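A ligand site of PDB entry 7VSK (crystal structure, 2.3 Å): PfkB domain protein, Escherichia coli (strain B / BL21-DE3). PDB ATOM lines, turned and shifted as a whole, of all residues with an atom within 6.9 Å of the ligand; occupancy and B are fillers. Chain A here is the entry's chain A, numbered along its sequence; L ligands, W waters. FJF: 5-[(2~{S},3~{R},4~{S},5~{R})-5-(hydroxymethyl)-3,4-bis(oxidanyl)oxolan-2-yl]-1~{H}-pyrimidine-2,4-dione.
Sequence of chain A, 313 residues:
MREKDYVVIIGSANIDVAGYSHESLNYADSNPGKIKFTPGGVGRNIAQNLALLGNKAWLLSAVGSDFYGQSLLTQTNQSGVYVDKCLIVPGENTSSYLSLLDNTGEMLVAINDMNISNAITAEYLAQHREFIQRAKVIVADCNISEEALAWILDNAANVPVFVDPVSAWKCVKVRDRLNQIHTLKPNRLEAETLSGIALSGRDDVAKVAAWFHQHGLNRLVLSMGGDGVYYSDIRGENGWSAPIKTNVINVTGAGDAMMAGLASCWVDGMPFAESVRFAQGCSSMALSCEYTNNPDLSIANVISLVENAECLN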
ATOM      1  N   SER A  12      19.965   6.988  30.409  1.00  0.00           N
ATOM      2  CA  SER A  12      19.494   5.738  30.949  1.00  0.00           C
ATOM      3  C   SER A  12      20.657   4.864  31.397  1.00  0.00           C
ATOM      4  O   SER A  12      21.790   4.996  30.920  1.00  0.00           O
ATOM      5  CB  SER A  12      18.622   4.986  29.941  1.00  0.00           C
ATOM      6  OG  SER A  12      19.358   4.700  28.768  1.00  0.00           O
ATOM      7  N   ALA A  13      20.352   3.966  32.339  1.00  0.00           N
ATOM      8  CA  ALA A  13      21.279   2.955  32.838  1.00  0.00           C
ATOM      9  C   ALA A  13      20.680   1.588  32.561  1.00  0.00           C
ATOM     10  O   ALA A  13      19.598   1.263  33.061  1.00  0.00           O
ATOM     11  CB  ALA A  13      21.538   3.127  34.337  1.00  0.00           C
ATOM     12  N   ASN A  14      21.362   0.804  31.739  1.00  0.00           N
ATOM     13  CA  ASN A  14      20.898  -0.511  31.352  1.00  0.00           C
ATOM     14  C   ASN A  14      21.804  -1.560  31.966  1.00  0.00           C
ATOM     15  O   ASN A  14      22.992  -1.345  32.163  1.00  0.00           O
ATOM     16  CB  ASN A  14      20.893  -0.683  29.841  1.00  0.00           C
ATOM     17  CG  ASN A  14      19.938   0.263  29.162  1.00  0.00           C
ATOM     18  OD1 ASN A  14      19.190   0.969  29.814  1.00  0.00           O
ATOM     19  ND2 ASN A  14      19.967   0.286  27.847  1.00  0.00           N
ATOM     20  N   ILE A  15      21.215  -2.717  32.257  1.00  0.00           N
ATOM     21  CA  ILE A  15      21.993  -3.941  32.379  1.00  0.00           C
ATOM     22  C   ILE A  15      22.100  -4.531  30.990  1.00  0.00           C
ATOM     23  O   ILE A  15      21.120  -4.965  30.398  1.00  0.00           O
ATOM     24  CB  ILE A  15      21.356  -4.920  33.373  1.00  0.00           C
ATOM     25  CG1 ILE A  15      21.295  -4.267  34.759  1.00  0.00           C
ATOM     26  CG2 ILE A  15      22.178  -6.200  33.404  1.00  0.00           C
ATOM     27  CD1 ILE A  15      20.255  -4.812  35.665  1.00  0.00           C
ATOM     28  N   ASP A  16      23.305  -4.498  30.440  1.00  0.00           N
ATOM     29  CA  ASP A  16      23.599  -5.184  29.199  1.00  0.00           C
ATOM     30  C   ASP A  16      23.774  -6.666  29.480  1.00  0.00           C
ATOM     31  O   ASP A  16      24.643  -7.054  30.268  1.00  0.00           O
ATOM     32  CB  ASP A  16      24.860  -4.621  28.572  1.00  0.00           C
ATOM     33  CG  ASP A  16      24.627  -3.289  27.920  1.00  0.00           C
ATOM     34  OD1 ASP A  16      23.554  -2.689  28.182  1.00  0.00           O
ATOM     35  OD2 ASP A  16      25.513  -2.861  27.152  1.00  0.00           O
ATOM     36  N   THR A  38      26.597  -6.669  32.178  1.00  0.00           N
ATOM     37  CA  THR A  38      27.423  -5.498  31.850  1.00  0.00           C
ATOM     38  C   THR A  38      26.652  -4.237  32.231  1.00  0.00           C
ATOM     39  O   THR A  38      25.432  -4.174  31.986  1.00  0.00           O
ATOM     40  CB  THR A  38      27.761  -5.469  30.364  1.00  0.00           C
ATOM     41  OG1 THR A  38      28.343  -6.715  29.971  1.00  0.00           O
ATOM     42  CG2 THR A  38      28.716  -4.355  30.037  1.00  0.00           C
ATOM     43  N   PRO A  39      27.305  -3.235  32.797  1.00  0.00           N
ATOM     44  CA  PRO A  39      26.637  -1.935  32.938  1.00  0.00           C
ATOM     45  C   PRO A  39      26.508  -1.274  31.584  1.00  0.00           C
ATOM     46  O   PRO A  39      27.336  -1.457  30.694  1.00  0.00           O
ATOM     47  CB  PRO A  39      27.555  -1.151  33.886  1.00  0.00           C
ATOM     48  CG  PRO A  39      28.898  -1.801  33.747  1.00  0.00           C
ATOM     49  CD  PRO A  39      28.669  -3.228  33.358  1.00  0.00           C
ATOM     50  N   GLY A  40      25.434  -0.530  31.418  1.00  0.00           N
ATOM     51  CA  GLY A  40      25.122   0.014  30.126  1.00  0.00           C
ATOM     52  C   GLY A  40      24.175   1.185  30.184  1.00  0.00           C
ATOM     53  O   GLY A  40      23.986   1.801  31.244  1.00  0.00           O
ATOM     54  N   GLY A  41      23.565   1.474  29.036  1.00  0.00           N
ATOM     55  CA  GLY A  41      22.814   2.698  28.854  1.00  0.00           C
ATOM     56  C   GLY A  41      23.768   3.716  28.285  1.00  0.00           C
ATOM     57  O   GLY A  41      24.939   3.719  28.687  1.00  0.00           O
ATOM     58  N   VAL A  42      23.346   4.586  27.357  1.00  0.00           N
ATOM     59  CA  VAL A  42      24.298   5.532  26.800  1.00  0.00           C
ATOM     60  C   VAL A  42      24.687   6.554  27.852  1.00  0.00           C
ATOM     61  O   VAL A  42      25.868   6.826  28.080  1.00  0.00           O
ATOM     62  CB  VAL A  42      23.744   6.186  25.521  1.00  0.00           C
ATOM     63  CG1 VAL A  42      24.652   7.328  25.137  1.00  0.00           C
ATOM     64  CG2 VAL A  42      23.699   5.186  24.406  1.00  0.00           C
ATOM     65  N   GLY A  43      23.699   7.090  28.572  1.00  0.00           N
ATOM     66  CA  GLY A  43      23.997   8.085  29.582  1.00  0.00           C
ATOM     67  C   GLY A  43      24.847   7.525  30.704  1.00  0.00           C
ATOM     68  O   GLY A  43      25.840   8.128  31.109  1.00  0.00           O
ATOM     69  N   ARG A  44      24.466   6.354  31.211  1.00  0.00           N
ATOM     70  CA  ARG A  44      25.239   5.785  32.311  1.00  0.00           C
ATOM     71  C   ARG A  44      26.668   5.487  31.866  1.00  0.00           C
ATOM     72  O   ARG A  44      27.615   5.681  32.631  1.00  0.00           O
ATOM     73  CB  ARG A  44      24.535   4.554  32.870  1.00  0.00           C
ATOM     74  CG  ARG A  44      25.216   3.953  34.092  1.00  0.00           C
ATOM     75  CD  ARG A  44      25.506   2.482  33.919  1.00  0.00           C
ATOM     76  NE  ARG A  44      26.561   2.207  32.958  1.00  0.00           N
ATOM     77  CZ  ARG A  44      27.856   2.061  33.235  1.00  0.00           C
ATOM     78  NH1 ARG A  44      28.319   2.210  34.460  1.00  0.00           N
ATOM     79  NH2 ARG A  44      28.707   1.739  32.267  1.00  0.00           N
ATOM     80  N   ASN A  45      26.849   5.071  30.617  1.00  0.00           N
ATOM     81  CA  ASN A  45      28.193   4.788  30.123  1.00  0.00           C
ATOM     82  C   ASN A  45      29.024   6.061  30.058  1.00  0.00           C
ATOM     83  O   ASN A  45      30.177   6.085  30.519  1.00  0.00           O
ATOM     84  CB  ASN A  45      28.145   4.128  28.754  1.00  0.00           C
ATOM     85  CG  ASN A  45      27.535   2.762  28.813  1.00  0.00           C
ATOM     86  OD1 ASN A  45      27.235   2.269  29.892  1.00  0.00           O
ATOM     87  ND2 ASN A  45      27.336   2.149  27.644  1.00  0.00           N
ATOM     88  N   SER A  96      17.224  -2.749  30.474  1.00  0.00           N
ATOM     89  CA  SER A  96      18.222  -3.744  30.125  1.00  0.00           C
ATOM     90  C   SER A  96      18.273  -3.852  28.608  1.00  0.00           C
ATOM     91  O   SER A  96      17.331  -3.488  27.898  1.00  0.00           O
ATOM     92  CB  SER A  96      17.929  -5.094  30.772  1.00  0.00           C
ATOM     93  OG  SER A  96      16.532  -5.335  30.895  1.00  0.00           O
ATOM     94  N   TYR A  97      19.400  -4.358  28.128  1.00  0.00           N
ATOM     95  CA  TYR A  97      19.677  -4.421  26.706  1.00  0.00           C
ATOM     96  C   TYR A  97      20.147  -5.851  26.431  1.00  0.00           C
ATOM     97  O   TYR A  97      21.334  -6.160  26.556  1.00  0.00           O
ATOM     98  CB  TYR A  97      20.703  -3.375  26.311  1.00  0.00           C
ATOM     99  CG  TYR A  97      21.046  -3.442  24.861  1.00  0.00           C
ATOM    100  CD1 TYR A  97      20.224  -2.875  23.899  1.00  0.00           C
ATOM    101  CD2 TYR A  97      22.198  -4.107  24.436  1.00  0.00           C
ATOM    102  CE1 TYR A  97      20.543  -2.949  22.559  1.00  0.00           C
ATOM    103  CE2 TYR A  97      22.529  -4.191  23.102  1.00  0.00           C
ATOM    104  CZ  TYR A  97      21.702  -3.617  22.163  1.00  0.00           C
ATOM    105  OH  TYR A  97      22.024  -3.703  20.831  1.00  0.00           O
ATOM    106  N   ASN A 112      15.391  -4.838  23.550  1.00  0.00           N
ATOM    107  CA  ASN A 112      15.625  -3.603  24.286  1.00  0.00           C
ATOM    108  C   ASN A 112      14.400  -3.299  25.149  1.00  0.00           C
ATOM    109  O   ASN A 112      13.305  -3.097  24.611  1.00  0.00           O
ATOM    110  CB  ASN A 112      15.917  -2.459  23.320  1.00  0.00           C
ATOM    111  CG  ASN A 112      15.721  -1.110  23.931  1.00  0.00           C
ATOM    112  OD1 ASN A 112      14.605  -0.593  23.993  1.00  0.00           O
ATOM    113  ND2 ASN A 112      16.809  -0.526  24.423  1.00  0.00           N
ATOM    114  N   MET A 114      13.262  -0.621  27.837  1.00  0.00           N
ATOM    115  CA  MET A 114      13.711   0.631  28.438  1.00  0.00           C
ATOM    116  C   MET A 114      12.572   1.577  28.743  1.00  0.00           C
ATOM    117  O   MET A 114      12.791   2.794  28.773  1.00  0.00           O
ATOM    118  CB  MET A 114      14.738   1.342  27.569  1.00  0.00           C
ATOM    119  CG  MET A 114      16.088   0.687  27.542  1.00  0.00           C
ATOM    120  SD  MET A 114      17.132   1.387  26.271  1.00  0.00           S
ATOM    121  CE  MET A 114      17.745   2.819  27.137  1.00  0.00           C
ATOM    122  N   SER A 117      13.066   4.268  31.187  1.00  0.00           N
ATOM    123  CA  SER A 117      13.685   5.485  30.699  1.00  0.00           C
ATOM    124  C   SER A 117      12.690   6.639  30.725  1.00  0.00           C
ATOM    125  O   SER A 117      13.048   7.799  30.972  1.00  0.00           O
ATOM    126  CB  SER A 117      14.214   5.238  29.282  1.00  0.00           C
ATOM    127  OG  SER A 117      15.521   5.753  29.126  1.00  0.00           O
ATOM    128  N   ASP A 141      21.261  12.063  26.974  1.00  0.00           N
ATOM    129  CA  ASP A 141      21.056  11.192  25.833  1.00  0.00           C
ATOM    130  C   ASP A 141      19.602  11.266  25.390  1.00  0.00           C
ATOM    131  O   ASP A 141      18.742  11.810  26.089  1.00  0.00           O
ATOM    132  CB  ASP A 141      21.502   9.738  26.133  1.00  0.00           C
ATOM    133  CG  ASP A 141      20.571   8.987  27.087  1.00  0.00           C
ATOM    134  OD1 ASP A 141      19.333   9.198  27.066  1.00  0.00           O
ATOM    135  OD2 ASP A 141      21.095   8.125  27.845  1.00  0.00           O
ATOM    136  N   CYS A 142      19.341  10.743  24.207  1.00  0.00           N
ATOM    137  CA  CYS A 142      17.994  10.753  23.676  1.00  0.00           C
ATOM    138  C   CYS A 142      17.215   9.474  23.998  1.00  0.00           C
ATOM    139  O   CYS A 142      16.296   9.115  23.254  1.00  0.00           O
ATOM    140  CB  CYS A 142      18.055  10.997  22.174  1.00  0.00           C
ATOM    141  SG  CYS A 142      18.790  12.617  21.859  1.00  0.00           S
ATOM    142  N   ASN A 143      17.550   8.779  25.086  1.00  0.00           N
ATOM    143  CA  ASN A 143      16.670   7.749  25.614  1.00  0.00           C
ATOM    144  C   ASN A 143      15.545   8.357  26.431  1.00  0.00           C
ATOM    145  O   ASN A 143      14.444   7.793  26.486  1.00  0.00           O
ATOM    146  CB  ASN A 143      17.441   6.766  26.501  1.00  0.00           C
ATOM    147  CG  ASN A 143      18.396   5.923  25.726  1.00  0.00           C
ATOM    148  OD1 ASN A 143      18.006   5.181  24.837  1.00  0.00           O
ATOM    149  ND2 ASN A 143      19.662   6.053  26.048  1.00  0.00           N
ATOM    150  N   VAL A 166      21.965   8.655  20.423  1.00  0.00           N
ATOM    151  CA  VAL A 166      21.660   7.274  20.798  1.00  0.00           C
ATOM    152  C   VAL A 166      21.334   6.409  19.585  1.00  0.00           C
ATOM    153  O   VAL A 166      22.002   5.404  19.360  1.00  0.00           O
ATOM    154  CB  VAL A 166      20.536   7.230  21.847  1.00  0.00           C
ATOM    155  CG1 VAL A 166      20.267   5.803  22.269  1.00  0.00           C
ATOM    156  CG2 VAL A 166      20.943   8.069  23.046  1.00  0.00           C
ATOM    157  N   SER A 167      20.332   6.773  18.796  1.00  0.00           N
ATOM    158  CA  SER A 167      20.032   6.009  17.590  1.00  0.00           C
ATOM    159  C   SER A 167      19.265   6.876  16.603  1.00  0.00           C
ATOM    160  O   SER A 167      18.793   7.963  16.936  1.00  0.00           O
ATOM    161  CB  SER A 167      19.211   4.749  17.915  1.00  0.00           C
ATOM    162  OG  SER A 167      17.903   5.106  18.327  1.00  0.00           O
ATOM    163  N   LYS A 170      15.781   7.351  18.155  1.00  0.00           N
ATOM    164  CA  LYS A 170      15.674   8.241  19.294  1.00  0.00           C
ATOM    165  C   LYS A 170      16.230   9.636  19.024  1.00  0.00           C
ATOM    166  O   LYS A 170      15.876  10.568  19.752  1.00  0.00           O
ATOM    167  CB  LYS A 170      16.384   7.642  20.509  1.00  0.00           C
ATOM    168  CG  LYS A 170      16.002   6.200  20.802  1.00  0.00           C
ATOM    169  CD  LYS A 170      16.149   5.836  22.275  1.00  0.00           C
ATOM    170  CE  LYS A 170      15.430   4.521  22.577  1.00  0.00           C
ATOM    171  NZ  LYS A 170      15.779   3.912  23.914  1.00  0.00           N
ATOM    172  N   ALA A 254      31.960   2.785  22.200  1.00  0.00           N
ATOM    173  CA  ALA A 254      32.930   3.638  21.520  1.00  0.00           C
ATOM    174  C   ALA A 254      32.399   5.062  21.540  1.00  0.00           C
ATOM    175  O   ALA A 254      33.028   5.954  22.097  1.00  0.00           O
ATOM    176  CB  ALA A 254      33.175   3.178  20.104  1.00  0.00           C
ATOM    177  N   GLY A 255      31.240   5.256  20.903  1.00  0.00           N
ATOM    178  CA  GLY A 255      30.561   6.536  20.908  1.00  0.00           C
ATOM    179  C   GLY A 255      30.334   7.027  22.324  1.00  0.00           C
ATOM    180  O   GLY A 255      30.191   8.231  22.559  1.00  0.00           O
ATOM    181  N   ASP A 256      30.314   6.106  23.284  1.00  0.00           N
ATOM    182  CA  ASP A 256      30.157   6.512  24.671  1.00  0.00           C
ATOM    183  C   ASP A 256      31.447   7.104  25.228  1.00  0.00           C
ATOM    184  O   ASP A 256      31.405   8.058  26.016  1.00  0.00           O
ATOM    185  CB  ASP A 256      29.693   5.330  25.509  1.00  0.00           C
ATOM    186  CG  ASP A 256      28.301   4.882  25.124  1.00  0.00           C
ATOM    187  OD1 ASP A 256      27.579   5.681  24.470  1.00  0.00           O
ATOM    188  OD2 ASP A 256      27.949   3.727  25.459  1.00  0.00           O
HETATM  189  O01 FJF L   1      18.145   2.461  22.739  1.00  0.00           O
HETATM  190  C02 FJF L   1      19.199   2.236  23.357  1.00  0.00           C
HETATM  191  N03 FJF L   1      19.956   1.110  23.082  1.00  0.00           N
HETATM  192  C04 FJF L   1      21.116   0.832  23.739  1.00  0.00           C
HETATM  193  C05 FJF L   1      21.558   1.715  24.717  1.00  0.00           C
HETATM  194  C06 FJF L   1      20.799   2.846  25.024  1.00  0.00           C
HETATM  195  O07 FJF L   1      21.180   3.633  25.890  1.00  0.00           O
HETATM  196  N08 FJF L   1      19.622   3.117  24.340  1.00  0.00           N
HETATM  197  C09 FJF L   1      22.826   1.466  25.485  1.00  0.00           C
HETATM  198  O10 FJF L   1      23.940   1.953  24.782  1.00  0.00           O
HETATM  199  C11 FJF L   1      25.107   1.182  25.150  1.00  0.00           C
HETATM  200  C12 FJF L   1      25.985   1.060  23.932  1.00  0.00           C
HETATM  201  O13 FJF L   1      26.524   2.329  23.555  1.00  0.00           O
HETATM  202  C14 FJF L   1      24.600  -0.135  25.731  1.00  0.00           C
HETATM  203  O15 FJF L   1      25.000  -0.231  27.094  1.00  0.00           O
HETATM  204  C16 FJF L   1      23.067  -0.024  25.697  1.00  0.00           C
HETATM  205  O17 FJF L   1      22.454  -0.457  26.906  1.00  0.00           O
HETATM  206  O   HOH W   1      16.972   2.998  20.113  1.00  0.00           O
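The side-chain amide oxygen of Asn 143 lies within hydrogen-bond range of a nitrogen (N08) of the ligand. The side-chain carboxylate of Asp 16 lies within hydrogen-bond range of an oxygen (O15) of the ligand (2.7 Å). O13 of the ligand sits at hydrogen-bond distance from OD2 of Asp 256, 2.8 Å away. The side-chain amide nitrogen (ND2) of Asn 14 lies within hydrogen-bond range of an oxygen (O17) of the ligand, 2.8 Å away. O07 of the ligand sits at hydrogen-bond distance from N of Val 42, 2.8 Å away. An oxygen (O15) of the ligand sits at hydrogen-bond distance from the backbone NH (N) of Gly 41, at 3.0 Å. The side-chain amino group of Lys 170 sits at hydrogen-bond distance from an oxygen (O01) of the ligand (3.0 Å). The side-chain amide nitrogen (ND2) of Asn 45 is in hydrogen-bond range of an oxygen (O15) of the ligand (3.4 Å). The side-chain sulfur (SD) of Met 114 sits close to a nitrogen (N08) of the ligand.
The side-chain hydroxyl (OG) of Ser 12 sits at hydrogen-bond distance from the side-chain amide nitrogen (ND2) of Asn 143, at 3.1 Å. The backbone NH (N) of Asp 16 lies within hydrogen-bond range of the backbone carbonyl oxygen (O) of Thr 38, 2.6 Å away. The side-chain carboxylate (OD2) of Asp 256 is in hydrogen-bond range of the side-chain amide nitrogen (ND2) of Asn 45, at 2.8 Å. ND2 of Asn 14 lies within hydrogen-bond range of SD of Met 114 (3.4 Å). N of Lys 170 is in hydrogen-bond range of OG of Ser 167 (3.1 Å). The side-chain sulfur (SD) of Met 114 sits at hydrogen-bond distance from the side-chain amide nitrogen (ND2) of Asn 112 (2.7 Å). The backbone NH (N) of Tyr 97 lies within hydrogen-bond range of the backbone carbonyl oxygen (O) of Ile 15 (2.9 Å). The side-chain carboxylate (OD2) of Asp 141 is in hydrogen-bond range of the backbone NH (N) of Ser 12 (3.0 Å).
Ser 12 touches the ligand. Gly 40 touches the ligand (CA to O15, 3.0 Å). Tyr 97 touches the ligand (CB to O17, 3.5 Å). Asn 112 touches the ligand. Val 166 touches the ligand. Hydrophobic or aromatic side chains within 4 Å of the ligand: Val 42, Tyr 97, Met 114 and Val 166. Of the 27 residues printed, 14 come within 4 Å of the ligand. The nearest printed residue that does not touch the ligand is Pro 39 (4.5 Å).
Water W1 bridges the side-chain hydroxyl (OG) of Ser 167 (2.9 Å) and an oxygen (O01) of the ligand (2.9 Å).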
